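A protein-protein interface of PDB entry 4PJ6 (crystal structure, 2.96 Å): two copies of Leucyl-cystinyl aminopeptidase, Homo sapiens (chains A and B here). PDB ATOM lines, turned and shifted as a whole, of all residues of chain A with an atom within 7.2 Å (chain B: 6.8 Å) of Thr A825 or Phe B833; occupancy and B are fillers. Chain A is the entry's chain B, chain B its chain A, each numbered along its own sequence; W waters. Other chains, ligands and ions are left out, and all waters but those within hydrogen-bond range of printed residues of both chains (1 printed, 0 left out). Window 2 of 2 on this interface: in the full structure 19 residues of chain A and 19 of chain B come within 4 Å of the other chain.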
ATOM      1  N   SER A 822     -32.793  26.271 -15.087  1.00  0.00           N
ATOM      2  CA  SER A 822     -32.700  24.854 -15.483  1.00  0.00           C
ATOM      3  C   SER A 822     -31.391  24.480 -16.263  1.00  0.00           C
ATOM      4  O   SER A 822     -31.381  23.694 -17.205  1.00  0.00           O
ATOM      5  CB  SER A 822     -34.000  24.390 -16.176  1.00  0.00           C
ATOM      6  OG  SER A 822     -34.364  25.234 -17.242  1.00  0.00           O
ATOM      7  N   THR A 823     -30.282  25.035 -15.824  1.00  0.00           N
ATOM      8  CA  THR A 823     -28.999  24.770 -16.426  1.00  0.00           C
ATOM      9  C   THR A 823     -27.961  24.532 -15.322  1.00  0.00           C
ATOM     10  O   THR A 823     -28.069  25.086 -14.204  1.00  0.00           O
ATOM     11  CB  THR A 823     -28.506  25.943 -17.343  1.00  0.00           C
ATOM     12  OG1 THR A 823     -27.917  27.009 -16.556  1.00  0.00           O
ATOM     13  CG2 THR A 823     -29.636  26.471 -18.260  1.00  0.00           C
ATOM     14  N   LYS A 824     -26.942  23.734 -15.672  1.00  0.00           N
ATOM     15  CA  LYS A 824     -25.873  23.351 -14.744  1.00  0.00           C
ATOM     16  C   LYS A 824     -25.076  24.576 -14.354  1.00  0.00           C
ATOM     17  O   LYS A 824     -24.570  24.666 -13.262  1.00  0.00           O
ATOM     18  CB  LYS A 824     -24.981  22.232 -15.337  1.00  0.00           C
ATOM     19  CG  LYS A 824     -25.785  20.985 -15.775  1.00  0.00           C
ATOM     20  CD  LYS A 824     -24.939  19.734 -16.042  1.00  0.00           C
ATOM     21  CE  LYS A 824     -24.717  18.845 -14.803  1.00  0.00           C
ATOM     22  NZ  LYS A 824     -23.447  18.040 -14.912  1.00  0.00           N
ATOM     23  N   THR A 825     -25.004  25.543 -15.247  1.00  0.00           N
ATOM     24  CA  THR A 825     -24.288  26.768 -14.951  1.00  0.00           C
ATOM     25  C   THR A 825     -25.051  27.550 -13.884  1.00  0.00           C
ATOM     26  O   THR A 825     -24.461  28.030 -12.926  1.00  0.00           O
ATOM     27  CB  THR A 825     -24.072  27.595 -16.228  1.00  0.00           C
ATOM     28  OG1 THR A 825     -23.580  26.736 -17.265  1.00  0.00           O
ATOM     29  CG2 THR A 825     -23.067  28.704 -15.989  1.00  0.00           C
ATOM     30  N   HIS A 826     -26.363  27.659 -14.038  1.00  0.00           N
ATOM     31  CA  HIS A 826     -27.127  28.378 -13.064  1.00  0.00           C
ATOM     32  C   HIS A 826     -26.982  27.693 -11.710  1.00  0.00           C
ATOM     33  O   HIS A 826     -26.718  28.364 -10.697  1.00  0.00           O
ATOM     34  CB  HIS A 826     -28.578  28.512 -13.512  1.00  0.00           C
ATOM     35  CG  HIS A 826     -28.812  29.686 -14.410  1.00  0.00           C
ATOM     36  ND1 HIS A 826     -28.590  30.986 -14.002  1.00  0.00           N
ATOM     37  CD2 HIS A 826     -29.235  29.764 -15.695  1.00  0.00           C
ATOM     38  CE1 HIS A 826     -28.866  31.810 -14.999  1.00  0.00           C
ATOM     39  NE2 HIS A 826     -29.255  31.095 -16.040  1.00  0.00           N
ATOM     40  N   LEU A 827     -27.136  26.358 -11.712  1.00  0.00           N
ATOM     41  CA  LEU A 827     -27.112  25.531 -10.503  1.00  0.00           C
ATOM     42  C   LEU A 827     -25.815  25.747  -9.748  1.00  0.00           C
ATOM     43  O   LEU A 827     -25.818  25.803  -8.506  1.00  0.00           O
ATOM     44  CB  LEU A 827     -27.205  24.063 -10.883  1.00  0.00           C
ATOM     45  CG  LEU A 827     -27.108  23.003  -9.789  1.00  0.00           C
ATOM     46  CD1 LEU A 827     -28.257  23.156  -8.796  1.00  0.00           C
ATOM     47  CD2 LEU A 827     -27.099  21.609 -10.408  1.00  0.00           C
ATOM     48  N   SER A 828     -24.714  25.863 -10.500  1.00  0.00           N
ATOM     49  CA  SER A 828     -23.393  26.072  -9.921  1.00  0.00           C
ATOM     50  C   SER A 828     -23.339  27.427  -9.252  1.00  0.00           C
ATOM     51  O   SER A 828     -22.916  27.514  -8.078  1.00  0.00           O
ATOM     52  CB  SER A 828     -22.286  25.964 -10.964  1.00  0.00           C
ATOM     53  OG  SER A 828     -22.318  24.707 -11.600  1.00  0.00           O
ATOM     54  N   GLU A 829     -23.793  28.455  -9.993  1.00  0.00           N
ATOM     55  CA  GLU A 829     -23.879  29.844  -9.529  1.00  0.00           C
ATOM     56  C   GLU A 829     -24.717  30.013  -8.284  1.00  0.00           C
ATOM     57  O   GLU A 829     -24.297  30.681  -7.350  1.00  0.00           O
ATOM     58  CB  GLU A 829     -24.465  30.722 -10.632  1.00  0.00           C
ATOM     59  CG  GLU A 829     -25.285  31.938 -10.154  1.00  0.00           C
ATOM     60  CD  GLU A 829     -26.232  32.530 -11.201  1.00  0.00           C
ATOM     61  OE1 GLU A 829     -26.614  33.708 -10.971  1.00  0.00           O
ATOM     62  OE2 GLU A 829     -26.607  31.849 -12.216  1.00  0.00           O
ATOM     63  N   VAL A 830     -25.906  29.415  -8.288  1.00  0.00           N
ATOM     64  CA  VAL A 830     -26.850  29.539  -7.170  1.00  0.00           C
ATOM     65  C   VAL A 830     -26.205  28.969  -5.941  1.00  0.00           C
ATOM     66  O   VAL A 830     -26.211  29.638  -4.900  1.00  0.00           O
ATOM     67  CB  VAL A 830     -28.267  28.944  -7.465  1.00  0.00           C
ATOM     68  CG1 VAL A 830     -29.117  28.888  -6.202  1.00  0.00           C
ATOM     69  CG2 VAL A 830     -28.982  29.758  -8.549  1.00  0.00           C
ATOM     70  N   GLN A 831     -25.604  27.775  -6.087  1.00  0.00           N
ATOM     71  CA  GLN A 831     -24.880  27.096  -4.982  1.00  0.00           C
ATOM     72  C   GLN A 831     -23.749  27.954  -4.440  1.00  0.00           C
ATOM     73  O   GLN A 831     -23.838  28.434  -3.310  1.00  0.00           O
ATOM     74  CB  GLN A 831     -24.317  25.750  -5.427  1.00  0.00           C
ATOM     75  CG  GLN A 831     -23.829  24.851  -4.289  1.00  0.00           C
ATOM     76  CD  GLN A 831     -23.568  23.456  -4.778  1.00  0.00           C
ATOM     77  OE1 GLN A 831     -22.879  23.262  -5.789  1.00  0.00           O
ATOM     78  NE2 GLN A 831     -24.147  22.468  -4.091  1.00  0.00           N
ATOM     79  N   ILE A 854     -33.493  22.980  -9.100  1.00  0.00           N
ATOM     80  CA  ILE A 854     -32.741  23.307 -10.321  1.00  0.00           C
ATOM     81  C   ILE A 854     -32.333  22.027 -11.037  1.00  0.00           C
ATOM     82  O   ILE A 854     -32.695  21.875 -12.214  1.00  0.00           O
ATOM     83  CB  ILE A 854     -31.570  24.320 -10.124  1.00  0.00           C
ATOM     84  CG1 ILE A 854     -32.083  25.595  -9.442  1.00  0.00           C
ATOM     85  CG2 ILE A 854     -30.888  24.639 -11.458  1.00  0.00           C
ATOM     86  CD1 ILE A 854     -31.055  26.619  -9.007  1.00  0.00           C
ATOM     87  N   ILE A 858     -33.134  20.592 -14.688  1.00  0.00           N
ATOM     88  CA  ILE A 858     -32.045  20.044 -15.511  1.00  0.00           C
ATOM     89  C   ILE A 858     -32.350  18.624 -16.003  1.00  0.00           C
ATOM     90  O   ILE A 858     -32.231  18.320 -17.220  1.00  0.00           O
ATOM     91  CB  ILE A 858     -30.685  20.062 -14.778  1.00  0.00           C
ATOM     92  CG1 ILE A 858     -30.304  21.492 -14.419  1.00  0.00           C
ATOM     93  CG2 ILE A 858     -29.618  19.548 -15.707  1.00  0.00           C
ATOM     94  CD1 ILE A 858     -29.224  21.606 -13.384  1.00  0.00           C
ATOM     95  N   TRP B 789     -24.087  38.967 -20.248  1.00  0.00           N
ATOM     96  CA  TRP B 789     -23.132  38.202 -19.469  1.00  0.00           C
ATOM     97  C   TRP B 789     -23.608  36.750 -19.262  1.00  0.00           C
ATOM     98  O   TRP B 789     -22.796  35.826 -19.301  1.00  0.00           O
ATOM     99  CB  TRP B 789     -22.788  38.895 -18.115  1.00  0.00           C
ATOM    100  CG  TRP B 789     -21.945  38.005 -17.146  1.00  0.00           C
ATOM    101  CD1 TRP B 789     -22.264  37.668 -15.877  1.00  0.00           C
ATOM    102  CD2 TRP B 789     -20.706  37.354 -17.435  1.00  0.00           C
ATOM    103  NE1 TRP B 789     -21.310  36.863 -15.344  1.00  0.00           N
ATOM    104  CE2 TRP B 789     -20.332  36.648 -16.274  1.00  0.00           C
ATOM    105  CE3 TRP B 789     -19.869  37.313 -18.549  1.00  0.00           C
ATOM    106  CZ2 TRP B 789     -19.145  35.889 -16.186  1.00  0.00           C
ATOM    107  CZ3 TRP B 789     -18.680  36.560 -18.467  1.00  0.00           C
ATOM    108  CH2 TRP B 789     -18.337  35.852 -17.296  1.00  0.00           C
ATOM    109  N   ASP B 790     -24.913  36.572 -19.048  1.00  0.00           N
ATOM    110  CA  ASP B 790     -25.556  35.241 -18.969  1.00  0.00           C
ATOM    111  C   ASP B 790     -25.396  34.501 -20.305  1.00  0.00           C
ATOM    112  O   ASP B 790     -25.123  33.312 -20.324  1.00  0.00           O
ATOM    113  CB  ASP B 790     -27.047  35.409 -18.616  1.00  0.00           C
ATOM    114  CG  ASP B 790     -27.734  34.114 -18.298  1.00  0.00           C
ATOM    115  OD1 ASP B 790     -27.443  33.517 -17.239  1.00  0.00           O
ATOM    116  OD2 ASP B 790     -28.613  33.715 -19.099  1.00  0.00           O
ATOM    117  N   VAL B 792     -23.059  34.932 -22.605  1.00  0.00           N
ATOM    118  CA  VAL B 792     -21.649  34.581 -22.626  1.00  0.00           C
ATOM    119  C   VAL B 792     -21.398  33.286 -21.798  1.00  0.00           C
ATOM    120  O   VAL B 792     -20.796  32.336 -22.291  1.00  0.00           O
ATOM    121  CB  VAL B 792     -20.786  35.768 -22.139  1.00  0.00           C
ATOM    122  CG1 VAL B 792     -19.343  35.347 -21.908  1.00  0.00           C
ATOM    123  CG2 VAL B 792     -20.840  36.893 -23.150  1.00  0.00           C
ATOM    124  N   LYS B 793     -21.920  33.253 -20.573  1.00  0.00           N
ATOM    125  CA  LYS B 793     -21.766  32.154 -19.632  1.00  0.00           C
ATOM    126  C   LYS B 793     -22.292  30.838 -20.192  1.00  0.00           C
ATOM    127  O   LYS B 793     -21.542  29.840 -20.256  1.00  0.00           O
ATOM    128  CB  LYS B 793     -22.465  32.462 -18.290  1.00  0.00           C
ATOM    129  CG  LYS B 793     -21.708  33.451 -17.409  1.00  0.00           C
ATOM    130  CD  LYS B 793     -22.182  33.369 -15.976  1.00  0.00           C
ATOM    131  CE  LYS B 793     -23.451  34.168 -15.679  1.00  0.00           C
ATOM    132  NZ  LYS B 793     -24.216  33.601 -14.518  1.00  0.00           N
ATOM    133  N   GLU B 794     -23.568  30.826 -20.578  1.00  0.00           N
ATOM    134  CA  GLU B 794     -24.282  29.605 -20.957  1.00  0.00           C
ATOM    135  C   GLU B 794     -23.861  29.121 -22.300  1.00  0.00           C
ATOM    136  O   GLU B 794     -24.127  27.980 -22.576  1.00  0.00           O
ATOM    137  CB  GLU B 794     -25.800  29.827 -21.007  1.00  0.00           C
ATOM    138  CG  GLU B 794     -26.515  30.080 -19.685  1.00  0.00           C
ATOM    139  CD  GLU B 794     -26.639  28.855 -18.820  1.00  0.00           C
ATOM    140  OE1 GLU B 794     -26.507  27.728 -19.357  1.00  0.00           O
ATOM    141  OE2 GLU B 794     -26.858  29.039 -17.595  1.00  0.00           O
ATOM    142  N   ASN B 795     -23.251  29.968 -23.139  1.00  0.00           N
ATOM    143  CA  ASN B 795     -22.903  29.596 -24.518  1.00  0.00           C
ATOM    144  C   ASN B 795     -21.409  29.520 -24.680  1.00  0.00           C
ATOM    145  O   ASN B 795     -20.889  29.434 -25.799  1.00  0.00           O
ATOM    146  CB  ASN B 795     -23.483  30.605 -25.527  1.00  0.00           C
ATOM    147  CG  ASN B 795     -24.929  30.334 -25.865  1.00  0.00           C
ATOM    148  OD1 ASN B 795     -25.257  29.523 -26.748  1.00  0.00           O
ATOM    149  ND2 ASN B 795     -25.804  30.982 -25.142  1.00  0.00           N
ATOM    150  N   TRP B 796     -20.723  29.514 -23.529  1.00  0.00           N
ATOM    151  CA  TRP B 796     -19.268  29.512 -23.435  1.00  0.00           C
ATOM    152  C   TRP B 796     -18.578  28.470 -24.288  1.00  0.00           C
ATOM    153  O   TRP B 796     -17.557  28.780 -24.911  1.00  0.00           O
ATOM    154  CB  TRP B 796     -18.828  29.364 -22.001  1.00  0.00           C
ATOM    155  CG  TRP B 796     -17.360  29.561 -21.834  1.00  0.00           C
ATOM    156  CD1 TRP B 796     -16.447  28.614 -21.470  1.00  0.00           C
ATOM    157  CD2 TRP B 796     -16.622  30.779 -22.019  1.00  0.00           C
ATOM    158  NE1 TRP B 796     -15.179  29.161 -21.410  1.00  0.00           N
ATOM    159  CE2 TRP B 796     -15.258  30.490 -21.739  1.00  0.00           C
ATOM    160  CE3 TRP B 796     -16.978  32.083 -22.370  1.00  0.00           C
ATOM    161  CZ2 TRP B 796     -14.250  31.463 -21.810  1.00  0.00           C
ATOM    162  CZ3 TRP B 796     -15.992  33.038 -22.466  1.00  0.00           C
ATOM    163  CH2 TRP B 796     -14.638  32.725 -22.185  1.00  0.00           C
ATOM    164  N   SER B 828     -17.221  37.831  -7.231  1.00  0.00           N
ATOM    165  CA  SER B 828     -17.314  36.460  -6.836  1.00  0.00           C
ATOM    166  C   SER B 828     -17.816  35.618  -7.997  1.00  0.00           C
ATOM    167  O   SER B 828     -17.147  34.648  -8.383  1.00  0.00           O
ATOM    168  CB  SER B 828     -18.232  36.308  -5.648  1.00  0.00           C
ATOM    169  OG  SER B 828     -17.779  37.096  -4.579  1.00  0.00           O
ATOM    170  N   GLU B 829     -18.969  35.986  -8.551  1.00  0.00           N
ATOM    171  CA  GLU B 829     -19.617  35.260  -9.648  1.00  0.00           C
ATOM    172  C   GLU B 829     -18.667  35.087 -10.848  1.00  0.00           C
ATOM    173  O   GLU B 829     -18.466  33.982 -11.393  1.00  0.00           O
ATOM    174  CB  GLU B 829     -20.860  36.048 -10.077  1.00  0.00           C
ATOM    175  CG  GLU B 829     -21.461  35.640 -11.421  1.00  0.00           C
ATOM    176  CD  GLU B 829     -22.588  36.551 -11.862  1.00  0.00           C
ATOM    177  OE1 GLU B 829     -23.008  36.393 -13.035  1.00  0.00           O
ATOM    178  OE2 GLU B 829     -23.039  37.416 -11.052  1.00  0.00           O
ATOM    179  N   VAL B 830     -18.077  36.197 -11.266  1.00  0.00           N
ATOM    180  CA  VAL B 830     -17.264  36.157 -12.449  1.00  0.00           C
ATOM    181  C   VAL B 830     -16.152  35.164 -12.209  1.00  0.00           C
ATOM    182  O   VAL B 830     -16.063  34.198 -12.942  1.00  0.00           O
ATOM    183  CB  VAL B 830     -16.809  37.559 -12.900  1.00  0.00           C
ATOM    184  CG1 VAL B 830     -15.909  37.450 -14.125  1.00  0.00           C
ATOM    185  CG2 VAL B 830     -18.046  38.408 -13.195  1.00  0.00           C
ATOM    186  N   GLN B 831     -15.376  35.363 -11.147  1.00  0.00           N
ATOM    187  CA  GLN B 831     -14.271  34.460 -10.811  1.00  0.00           C
ATOM    188  C   GLN B 831     -14.732  33.016 -10.802  1.00  0.00           C
ATOM    189  O   GLN B 831     -14.171  32.168 -11.490  1.00  0.00           O
ATOM    190  CB  GLN B 831     -13.675  34.798  -9.435  1.00  0.00           C
ATOM    191  CG  GLN B 831     -12.424  34.012  -9.064  1.00  0.00           C
ATOM    192  CD  GLN B 831     -11.596  34.699  -8.014  1.00  0.00           C
ATOM    193  OE1 GLN B 831     -12.116  35.391  -7.139  1.00  0.00           O
ATOM    194  NE2 GLN B 831     -10.292  34.526  -8.102  1.00  0.00           N
ATOM    195  N   ALA B 832     -15.771  32.758 -10.016  1.00  0.00           N
ATOM    196  CA  ALA B 832     -16.329  31.425  -9.857  1.00  0.00           C
ATOM    197  C   ALA B 832     -16.432  30.767 -11.221  1.00  0.00           C
ATOM    198  O   ALA B 832     -15.860  29.709 -11.431  1.00  0.00           O
ATOM    199  CB  ALA B 832     -17.706  31.494  -9.150  1.00  0.00           C
ATOM    200  N   PHE B 833     -17.130  31.418 -12.146  1.00  0.00           N
ATOM    201  CA  PHE B 833     -17.422  30.863 -13.458  1.00  0.00           C
ATOM    202  C   PHE B 833     -16.183  30.432 -14.233  1.00  0.00           C
ATOM    203  O   PHE B 833     -16.193  29.400 -14.884  1.00  0.00           O
ATOM    204  CB  PHE B 833     -18.239  31.858 -14.281  1.00  0.00           C
ATOM    205  CG  PHE B 833     -18.472  31.429 -15.688  1.00  0.00           C
ATOM    206  CD1 PHE B 833     -19.484  30.555 -15.994  1.00  0.00           C
ATOM    207  CD2 PHE B 833     -17.669  31.912 -16.700  1.00  0.00           C
ATOM    208  CE1 PHE B 833     -19.700  30.165 -17.300  1.00  0.00           C
ATOM    209  CE2 PHE B 833     -17.878  31.535 -18.008  1.00  0.00           C
ATOM    210  CZ  PHE B 833     -18.901  30.665 -18.311  1.00  0.00           C
ATOM    211  N   PHE B 834     -15.127  31.212 -14.206  1.00  0.00           N
ATOM    212  CA  PHE B 834     -13.975  30.781 -14.937  1.00  0.00           C
ATOM    213  C   PHE B 834     -13.227  29.638 -14.206  1.00  0.00           C
ATOM    214  O   PHE B 834     -12.713  28.703 -14.853  1.00  0.00           O
ATOM    215  CB  PHE B 834     -13.087  31.962 -15.224  1.00  0.00           C
ATOM    216  CG  PHE B 834     -13.673  32.903 -16.196  1.00  0.00           C
ATOM    217  CD1 PHE B 834     -13.823  32.529 -17.521  1.00  0.00           C
ATOM    218  CD2 PHE B 834     -14.097  34.171 -15.788  1.00  0.00           C
ATOM    219  CE1 PHE B 834     -14.369  33.411 -18.438  1.00  0.00           C
ATOM    220  CE2 PHE B 834     -14.642  35.063 -16.701  1.00  0.00           C
ATOM    221  CZ  PHE B 834     -14.778  34.679 -18.030  1.00  0.00           C
ATOM    222  N   GLU B 835     -13.197  29.706 -12.864  1.00  0.00           N
ATOM    223  CA  GLU B 835     -12.694  28.619 -12.032  1.00  0.00           C
ATOM    224  C   GLU B 835     -13.475  27.347 -12.339  1.00  0.00           C
ATOM    225  O   GLU B 835     -12.922  26.257 -12.265  1.00  0.00           O
ATOM    226  CB  GLU B 835     -12.807  28.951 -10.549  1.00  0.00           C
ATOM    227  CG  GLU B 835     -11.684  29.828 -10.015  1.00  0.00           C
ATOM    228  CD  GLU B 835     -12.012  30.432  -8.645  1.00  0.00           C
ATOM    229  OE1 GLU B 835     -12.894  29.889  -7.927  1.00  0.00           O
ATOM    230  OE2 GLU B 835     -11.387  31.462  -8.278  1.00  0.00           O
ATOM    231  N   ASN B 836     -14.744  27.479 -12.704  1.00  0.00           N
ATOM    232  CA  ASN B 836     -15.574  26.313 -12.992  1.00  0.00           C
ATOM    233  C   ASN B 836     -15.353  25.788 -14.376  1.00  0.00           C
ATOM    234  O   ASN B 836     -15.956  24.787 -14.740  1.00  0.00           O
ATOM    235  CB  ASN B 836     -17.065  26.607 -12.831  1.00  0.00           C
ATOM    236  CG  ASN B 836     -17.494  26.671 -11.394  1.00  0.00           C
ATOM    237  OD1 ASN B 836     -17.646  25.643 -10.755  1.00  0.00           O
ATOM    238  ND2 ASN B 836     -17.697  27.893 -10.869  1.00  0.00           N
ATOM    239  N   GLN B 837     -14.530  26.466 -15.167  1.00  0.00           N
ATOM    240  CA  GLN B 837     -14.259  25.972 -16.511  1.00  0.00           C
ATOM    241  C   GLN B 837     -13.064  25.031 -16.432  1.00  0.00           C
ATOM    242  O   GLN B 837     -13.166  23.837 -16.709  1.00  0.00           O
ATOM    243  CB  GLN B 837     -13.991  27.112 -17.512  1.00  0.00           C
ATOM    244  CG  GLN B 837     -15.131  28.095 -17.686  1.00  0.00           C
ATOM    245  CD  GLN B 837     -16.464  27.409 -17.856  1.00  0.00           C
ATOM    246  OE1 GLN B 837     -16.777  26.889 -18.931  1.00  0.00           O
ATOM    247  NE2 GLN B 837     -17.261  27.402 -16.793  1.00  0.00           N
ATOM    248  N   SER B 838     -11.938  25.593 -16.028  1.00  0.00           N
ATOM    249  CA  SER B 838     -10.663  24.903 -15.946  1.00  0.00           C
ATOM    250  C   SER B 838      -9.800  25.928 -15.211  1.00  0.00           C
ATOM    251  O   SER B 838     -10.289  27.019 -14.839  1.00  0.00           O
ATOM    252  CB  SER B 838     -10.096  24.603 -17.362  1.00  0.00           C
ATOM    253  OG  SER B 838      -9.533  25.749 -17.988  1.00  0.00           O
ATOM    254  N   THR B 841      -8.292  28.432 -18.492  1.00  0.00           N
ATOM    255  CA  THR B 841      -9.205  29.549 -18.872  1.00  0.00           C
ATOM    256  C   THR B 841      -9.168  30.674 -17.810  1.00  0.00           C
ATOM    257  O   THR B 841      -9.155  31.856 -18.162  1.00  0.00           O
ATOM    258  CB  THR B 841     -10.669  29.092 -19.066  1.00  0.00           C
ATOM    259  OG1 THR B 841     -11.153  28.556 -17.834  1.00  0.00           O
ATOM    260  CG2 THR B 841     -10.782  28.031 -20.154  1.00  0.00           C
ATOM    261  N   PHE B 842      -9.133  30.292 -16.531  1.00  0.00           N
ATOM    262  CA  PHE B 842      -9.064  31.222 -15.404  1.00  0.00           C
ATOM    263  C   PHE B 842      -7.698  31.925 -15.271  1.00  0.00           C
ATOM    264  O   PHE B 842      -7.564  32.889 -14.512  1.00  0.00           O
ATOM    265  CB  PHE B 842      -9.443  30.471 -14.118  1.00  0.00           C
ATOM    266  CG  PHE B 842      -9.182  31.234 -12.839  1.00  0.00           C
ATOM    267  CD1 PHE B 842     -10.072  32.202 -12.402  1.00  0.00           C
ATOM    268  CD2 PHE B 842      -8.065  30.952 -12.045  1.00  0.00           C
ATOM    269  CE1 PHE B 842      -9.851  32.897 -11.215  1.00  0.00           C
ATOM    270  CE2 PHE B 842      -7.842  31.643 -10.853  1.00  0.00           C
ATOM    271  CZ  PHE B 842      -8.737  32.619 -10.439  1.00  0.00           C
HETATM  272  O   HOH W   1     -24.975  25.290 -18.920  1.00  0.00           O
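Thr A825 touches Glu B794.
Thr A825 touches Phe B833.
CD2 of His A826 touches OE2 of Glu B794 (3.1 Å).
Water W1 lies within hydrogen-bond range of OG1 of Thr A825 and OE1 of Glu B794.
4 positions are printed for both chains.
The side-chain carboxylate of Asp B790 sits close to a ring nitrogen (NE2) of His A826 (3.3 Å).
OE2 of Glu A829 lies within salt-bridge range of NZ of Lys B793.
The side-chain carboxylate (OE2) of Glu B794 sits at hydrogen-bond distance from the side-chain hydroxyl (OG1) of Thr A823.
The side-chain amino group of Lys B793 is in salt-bridge range of the side-chain carboxylate of Glu B829, at 3.4 Å.
The backbone carbonyl oxygen of Phe B833 is in hydrogen-bond range of the side-chain amide nitrogen of Gln B837 (3.0 Å).
The side-chain hydroxyl (OG1) of Thr A823 is in hydrogen-bond range of the backbone NH (N) of His A826, 3.0 Å away.
The side-chain carboxylate (OE2) of Glu A829 is in hydrogen-bond range of a ring nitrogen (ND1) of His A826, at 2.8 Å.
Hydrophobic or aromatic side chains of chain B that line the printed part of chain A: Phe B833.
Hydrophobic or aromatic side chains of chain A within 4 Å of the printed part of chain B: His A826.
Along chain A the printed residues that touch a printed residue of chain B span positions 823 to 829.
Among the printed residues, 6 pairs touch across the chains.
Printed residues of chain B within 4 Å of Thr A823: Glu B794 (2.5 Å).
Thr A825 touches just these residues of chain B: Glu B794 (3.4 Å) and Phe B833 (3.9 Å).
Printed residues of chain B within 4 Å of Glu A829: Lys B793 (3.8 Å).
Of the printed residues of chain A, Lys B793 touches Glu A829 (3.8 Å).
Of the printed residues of chain A, Glu B794 touches Thr A823, Thr A825 and His A826.
No residue of chain A comes within 4 Å of Ala B832.
Of chain A, only Thr A825 (3.9 Å) comes within 4 Å of Phe B833.
The nearest residue of chain B that does not touch Thr A825 is Lys B793 (4.4 Å).
The nearest printed residue of chain A that does not touch Phe B833 is Glu A829 (7.3 Å).
The nearest printed residue of chain B that does not touch His A826 is Lys B793 (5.0 Å).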
